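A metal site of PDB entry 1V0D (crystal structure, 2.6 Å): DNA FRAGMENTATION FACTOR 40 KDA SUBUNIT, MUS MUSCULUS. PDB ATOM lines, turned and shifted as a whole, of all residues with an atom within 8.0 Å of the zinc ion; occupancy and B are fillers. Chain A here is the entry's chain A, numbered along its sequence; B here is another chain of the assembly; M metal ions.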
ATOM      1  N   SER A 228      25.640  11.414  -9.039  1.00  0.00           N
ATOM      2  CA  SER A 228      24.854  12.213  -9.975  1.00  0.00           C
ATOM      3  C   SER A 228      23.423  11.790  -9.929  1.00  0.00           C
ATOM      4  O   SER A 228      23.103  10.599  -9.925  1.00  0.00           O
ATOM      5  CB  SER A 228      25.370  12.028 -11.403  1.00  0.00           C
ATOM      6  OG  SER A 228      26.581  12.741 -11.608  1.00  0.00           O
ATOM      7  N   CYS A 229      22.520  12.759  -9.884  1.00  0.00           N
ATOM      8  CA  CYS A 229      21.108  12.436  -9.865  1.00  0.00           C
ATOM      9  C   CYS A 229      20.821  11.711 -11.175  1.00  0.00           C
ATOM     10  O   CYS A 229      21.298  12.130 -12.237  1.00  0.00           O
ATOM     11  CB  CYS A 229      20.271  13.710  -9.783  1.00  0.00           C
ATOM     12  SG  CYS A 229      18.508  13.402  -9.673  1.00  0.00           S
ATOM     13  N   GLN A 230      20.080  10.614 -11.125  1.00  0.00           N
ATOM     14  CA  GLN A 230      19.760   9.901 -12.345  1.00  0.00           C
ATOM     15  C   GLN A 230      18.415  10.382 -12.909  1.00  0.00           C
ATOM     16  O   GLN A 230      17.805   9.713 -13.739  1.00  0.00           O
ATOM     17  CB  GLN A 230      19.682   8.405 -12.079  1.00  0.00           C
ATOM     18  CG  GLN A 230      20.899   7.839 -11.385  1.00  0.00           C
ATOM     19  CD  GLN A 230      20.849   6.321 -11.303  1.00  0.00           C
ATOM     20  OE1 GLN A 230      21.303   5.712 -10.325  1.00  0.00           O
ATOM     21  NE2 GLN A 230      20.302   5.701 -12.345  1.00  0.00           N
ATOM     22  N   GLY A 231      17.965  11.547 -12.447  1.00  0.00           N
ATOM     23  CA  GLY A 231      16.696  12.118 -12.899  1.00  0.00           C
ATOM     24  C   GLY A 231      15.484  11.331 -12.436  1.00  0.00           C
ATOM     25  O   GLY A 231      15.639  10.220 -11.932  1.00  0.00           O
ATOM     26  N   PRO A 232      14.271  11.861 -12.590  1.00  0.00           N
ATOM     27  CA  PRO A 232      13.113  11.073 -12.147  1.00  0.00           C
ATOM     28  C   PRO A 232      13.015   9.700 -12.826  1.00  0.00           C
ATOM     29  O   PRO A 232      13.683   9.429 -13.818  1.00  0.00           O
ATOM     30  CB  PRO A 232      11.925  11.995 -12.441  1.00  0.00           C
ATOM     31  CG  PRO A 232      12.424  12.875 -13.541  1.00  0.00           C
ATOM     32  CD  PRO A 232      13.845  13.157 -13.140  1.00  0.00           C
ATOM     33  N   SER A 237      17.637  11.161 -17.845  1.00  0.00           N
ATOM     34  CA  SER A 237      18.670  11.836 -17.062  1.00  0.00           C
ATOM     35  C   SER A 237      18.129  13.027 -16.261  1.00  0.00           C
ATOM     36  O   SER A 237      16.983  13.422 -16.442  1.00  0.00           O
ATOM     37  CB  SER A 237      19.761  12.328 -18.004  1.00  0.00           C
ATOM     38  OG  SER A 237      19.208  13.125 -19.038  1.00  0.00           O
ATOM     39  N   CYS A 238      18.963  13.583 -15.387  1.00  0.00           N
ATOM     40  CA  CYS A 238      18.563  14.716 -14.550  1.00  0.00           C
ATOM     41  C   CYS A 238      18.721  16.021 -15.313  1.00  0.00           C
ATOM     42  O   CYS A 238      19.836  16.465 -15.589  1.00  0.00           O
ATOM     43  CB  CYS A 238      19.409  14.773 -13.271  1.00  0.00           C
ATOM     44  SG  CYS A 238      19.130  16.237 -12.229  1.00  0.00           S
ATOM     45  N   LEU A 239      17.600  16.649 -15.629  1.00  0.00           N
ATOM     46  CA  LEU A 239      17.628  17.908 -16.370  1.00  0.00           C
ATOM     47  C   LEU A 239      18.304  19.038 -15.608  1.00  0.00           C
ATOM     48  O   LEU A 239      18.858  19.951 -16.219  1.00  0.00           O
ATOM     49  CB  LEU A 239      16.203  18.315 -16.740  1.00  0.00           C
ATOM     50  CG  LEU A 239      15.512  17.268 -17.627  1.00  0.00           C
ATOM     51  CD1 LEU A 239      13.997  17.504 -17.667  1.00  0.00           C
ATOM     52  CD2 LEU A 239      16.148  17.307 -19.023  1.00  0.00           C
ATOM     53  N   SER A 240      18.275  18.988 -14.285  1.00  0.00           N
ATOM     54  CA  SER A 240      18.888  20.035 -13.462  1.00  0.00           C
ATOM     55  C   SER A 240      20.371  19.734 -13.241  1.00  0.00           C
ATOM     56  O   SER A 240      21.141  20.615 -12.884  1.00  0.00           O
ATOM     57  CB  SER A 240      18.177  20.135 -12.116  1.00  0.00           C
ATOM     58  OG  SER A 240      16.779  20.243 -12.286  1.00  0.00           O
ATOM     59  N   LYS A 241      20.744  18.474 -13.467  1.00  0.00           N
ATOM     60  CA  LYS A 241      22.121  18.025 -13.303  1.00  0.00           C
ATOM     61  C   LYS A 241      22.603  18.096 -11.862  1.00  0.00           C
ATOM     62  O   LYS A 241      23.657  18.655 -11.566  1.00  0.00           O
ATOM     63  CB  LYS A 241      23.040  18.832 -14.201  1.00  0.00           C
ATOM     64  CG  LYS A 241      22.779  18.597 -15.662  1.00  0.00           C
ATOM     65  CD  LYS A 241      23.918  19.140 -16.502  1.00  0.00           C
ATOM     66  CE  LYS A 241      23.702  18.847 -17.968  1.00  0.00           C
ATOM     67  NZ  LYS A 241      24.832  19.419 -18.774  1.00  0.00           N
ATOM     68  N   HIS A 242      21.809  17.514 -10.968  1.00  0.00           N
ATOM     69  CA  HIS A 242      22.105  17.475  -9.542  1.00  0.00           C
ATOM     70  C   HIS A 242      23.251  16.533  -9.243  1.00  0.00           C
ATOM     71  O   HIS A 242      23.313  15.428  -9.784  1.00  0.00           O
ATOM     72  CB  HIS A 242      20.894  16.955  -8.767  1.00  0.00           C
ATOM     73  CG  HIS A 242      19.666  17.792  -8.925  1.00  0.00           C
ATOM     74  ND1 HIS A 242      18.436  17.244  -9.194  1.00  0.00           N
ATOM     75  CD2 HIS A 242      19.467  19.116  -8.749  1.00  0.00           C
ATOM     76  CE1 HIS A 242      17.519  18.203  -9.186  1.00  0.00           C
ATOM     77  NE2 HIS A 242      18.122  19.342  -8.917  1.00  0.00           N
ATOM     78  N   SER A 243      24.167  16.962  -8.382  1.00  0.00           N
ATOM     79  CA  SER A 243      25.282  16.103  -7.970  1.00  0.00           C
ATOM     80  C   SER A 243      25.497  16.351  -6.483  1.00  0.00           C
ATOM     81  O   SER A 243      24.895  17.252  -5.904  1.00  0.00           O
ATOM     82  CB  SER A 243      26.548  16.393  -8.772  1.00  0.00           C
ATOM     83  OG  SER A 243      27.136  17.631  -8.412  1.00  0.00           O
ATOM     84  N   TRP A 259      18.590  12.513  -0.463  1.00  0.00           N
ATOM     85  CA  TRP A 259      18.687  11.840  -1.756  1.00  0.00           C
ATOM     86  C   TRP A 259      18.099  10.466  -1.551  1.00  0.00           C
ATOM     87  O   TRP A 259      18.450   9.768  -0.603  1.00  0.00           O
ATOM     88  CB  TRP A 259      20.139  11.725  -2.206  1.00  0.00           C
ATOM     89  CG  TRP A 259      20.607  12.989  -2.806  1.00  0.00           C
ATOM     90  CD1 TRP A 259      20.684  14.204  -2.196  1.00  0.00           C
ATOM     91  CD2 TRP A 259      21.097  13.184  -4.136  1.00  0.00           C
ATOM     92  NE1 TRP A 259      21.191  15.145  -3.068  1.00  0.00           N
ATOM     93  CE2 TRP A 259      21.455  14.543  -4.269  1.00  0.00           C
ATOM     94  CE3 TRP A 259      21.272  12.326  -5.236  1.00  0.00           C
ATOM     95  CZ2 TRP A 259      21.974  15.069  -5.455  1.00  0.00           C
ATOM     96  CZ3 TRP A 259      21.785  12.845  -6.417  1.00  0.00           C
ATOM     97  CH2 TRP A 259      22.129  14.213  -6.507  1.00  0.00           C
ATOM     98  N   LEU A 302      19.009   6.582  -8.215  1.00  0.00           N
ATOM     99  CA  LEU A 302      19.444   7.460  -7.136  1.00  0.00           C
ATOM    100  C   LEU A 302      19.067   8.871  -7.525  1.00  0.00           C
ATOM    101  O   LEU A 302      19.681   9.456  -8.410  1.00  0.00           O
ATOM    102  CB  LEU A 302      20.957   7.374  -6.930  1.00  0.00           C
ATOM    103  CG  LEU A 302      21.553   8.361  -5.920  1.00  0.00           C
ATOM    104  CD1 LEU A 302      21.023   8.081  -4.521  1.00  0.00           C
ATOM    105  CD2 LEU A 302      23.065   8.255  -5.938  1.00  0.00           C
ATOM    106  N   VAL A 303      18.056   9.430  -6.870  1.00  0.00           N
ATOM    107  CA  VAL A 303      17.608  10.782  -7.197  1.00  0.00           C
ATOM    108  C   VAL A 303      17.674  11.803  -6.083  1.00  0.00           C
ATOM    109  O   VAL A 303      17.499  11.485  -4.900  1.00  0.00           O
ATOM    110  CB  VAL A 303      16.128  10.810  -7.706  1.00  0.00           C
ATOM    111  CG1 VAL A 303      15.946   9.874  -8.872  1.00  0.00           C
ATOM    112  CG2 VAL A 303      15.195  10.432  -6.568  1.00  0.00           C
ATOM    113  N   HIS A 304      17.908  13.039  -6.493  1.00  0.00           N
ATOM    114  CA  HIS A 304      17.936  14.189  -5.610  1.00  0.00           C
ATOM    115  C   HIS A 304      16.459  14.344  -5.274  1.00  0.00           C
ATOM    116  O   HIS A 304      15.605  13.874  -6.016  1.00  0.00           O
ATOM    117  CB  HIS A 304      18.477  15.389  -6.396  1.00  0.00           C
ATOM    118  CG  HIS A 304      18.259  16.726  -5.753  1.00  0.00           C
ATOM    119  ND1 HIS A 304      17.012  17.315  -5.671  1.00  0.00           N
ATOM    120  CD2 HIS A 304      19.144  17.633  -5.285  1.00  0.00           C
ATOM    121  CE1 HIS A 304      17.146  18.530  -5.172  1.00  0.00           C
ATOM    122  NE2 HIS A 304      18.419  18.749  -4.939  1.00  0.00           N
ATOM    123  N   ILE A 305      16.132  14.980  -4.156  1.00  0.00           N
ATOM    124  CA  ILE A 305      14.741  15.094  -3.762  1.00  0.00           C
ATOM    125  C   ILE A 305      13.814  15.778  -4.775  1.00  0.00           C
ATOM    126  O   ILE A 305      12.615  15.479  -4.840  1.00  0.00           O
ATOM    127  CB  ILE A 305      14.625  15.796  -2.378  1.00  0.00           C
ATOM    128  CG1 ILE A 305      13.170  15.748  -1.908  1.00  0.00           C
ATOM    129  CG2 ILE A 305      15.160  17.225  -2.475  1.00  0.00           C
ATOM    130  CD1 ILE A 305      12.966  16.349  -0.551  1.00  0.00           C
ATOM    131  N   ALA A 306      14.359  16.687  -5.573  1.00  0.00           N
ATOM    132  CA  ALA A 306      13.557  17.404  -6.569  1.00  0.00           C
ATOM    133  C   ALA A 306      13.205  16.522  -7.772  1.00  0.00           C
ATOM    134  O   ALA A 306      12.378  16.897  -8.618  1.00  0.00           O
ATOM    135  CB  ALA A 306      14.293  18.664  -7.028  1.00  0.00           C
ATOM    136  N   CYS A 307      13.834  15.359  -7.856  1.00  0.00           N
ATOM    137  CA  CYS A 307      13.612  14.424  -8.937  1.00  0.00           C
ATOM    138  C   CYS A 307      13.024  13.142  -8.395  1.00  0.00           C
ATOM    139  O   CYS A 307      13.205  12.082  -8.979  1.00  0.00           O
ATOM    140  CB  CYS A 307      14.912  14.101  -9.676  1.00  0.00           C
ATOM    141  SG  CYS A 307      15.586  15.474 -10.588  1.00  0.00           S
ATOM    142  N   HIS A 308      12.350  13.225  -7.260  1.00  0.00           N
ATOM    143  CA  HIS A 308      11.713  12.050  -6.691  1.00  0.00           C
ATOM    144  C   HIS A 308      10.234  12.293  -6.831  1.00  0.00           C
ATOM    145  O   HIS A 308       9.618  12.895  -5.967  1.00  0.00           O
ATOM    146  CB  HIS A 308      12.040  11.882  -5.212  1.00  0.00           C
ATOM    147  CG  HIS A 308      11.505  10.614  -4.619  1.00  0.00           C
ATOM    148  ND1 HIS A 308      11.500  10.357  -3.262  1.00  0.00           N
ATOM    149  CD2 HIS A 308      10.990   9.501  -5.196  1.00  0.00           C
ATOM    150  CE1 HIS A 308      11.018   9.155  -3.033  1.00  0.00           C
ATOM    151  NE2 HIS A 308      10.702   8.607  -4.196  1.00  0.00           N
ATOM    152  N   ARG B 250      10.921  26.256  -7.830  1.00  0.00           N
ATOM    153  CA  ARG B 250      10.274  24.973  -7.612  1.00  0.00           C
ATOM    154  C   ARG B 250      11.116  24.091  -6.704  1.00  0.00           C
ATOM    155  O   ARG B 250      10.620  23.531  -5.730  1.00  0.00           O
ATOM    156  CB  ARG B 250      10.042  24.251  -8.934  1.00  0.00           C
ATOM    157  CG  ARG B 250       9.594  22.825  -8.731  1.00  0.00           C
ATOM    158  CD  ARG B 250       9.422  22.055 -10.019  1.00  0.00           C
ATOM    159  NE  ARG B 250       9.075  20.671  -9.698  1.00  0.00           N
ATOM    160  CZ  ARG B 250       9.963  19.681  -9.608  1.00  0.00           C
ATOM    161  NH1 ARG B 250      11.266  19.903  -9.828  1.00  0.00           N
ATOM    162  NH2 ARG B 250       9.554  18.475  -9.235  1.00  0.00           N
ATOM    163  N   GLU B 251      12.385  23.968  -7.027  1.00  0.00           N
ATOM    164  CA  GLU B 251      13.300  23.152  -6.241  1.00  0.00           C
ATOM    165  C   GLU B 251      13.381  23.706  -4.813  1.00  0.00           C
ATOM    166  O   GLU B 251      13.548  22.957  -3.853  1.00  0.00           O
ATOM    167  CB  GLU B 251      14.680  23.150  -6.874  1.00  0.00           C
ATOM    168  CG  GLU B 251      15.692  22.295  -6.154  1.00  0.00           C
ATOM    169  CD  GLU B 251      16.938  22.057  -7.001  1.00  0.00           C
ATOM    170  OE1 GLU B 251      16.788  21.532  -8.127  1.00  0.00           O
ATOM    171  OE2 GLU B 251      18.045  22.412  -6.531  1.00  0.00           O
HETATM  172 ZN    ZN M   1      17.795  15.523 -10.449  1.00  0.00          ZN
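A ring nitrogen (NE2) of His 242 lies within hydrogen-bond range of the side-chain carboxylate (OE1) of Glu 251 of chain B, at 2.7 Å.
The side-chain sulfur (SG) of Cys 238 sits close to the backbone NH (N) of Ser 240 (3.5 Å).
The side-chain sulfur of Cys 238 sits close to the backbone NH of Lys 241 (3.0 Å).
The backbone NH of His 304 lies close to the side-chain sulfur of Cys 229, at 3.3 Å.
SG of Cys 229 lies close to N of Gly 231 (3.4 Å).
The zinc ion is bound by SG of Cys 307, ND1 of His 242, SG of Cys 238 and SG of Cys 229.
The nearest printed residue that does not touch the zinc ion is His 304 (4.1 Å).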
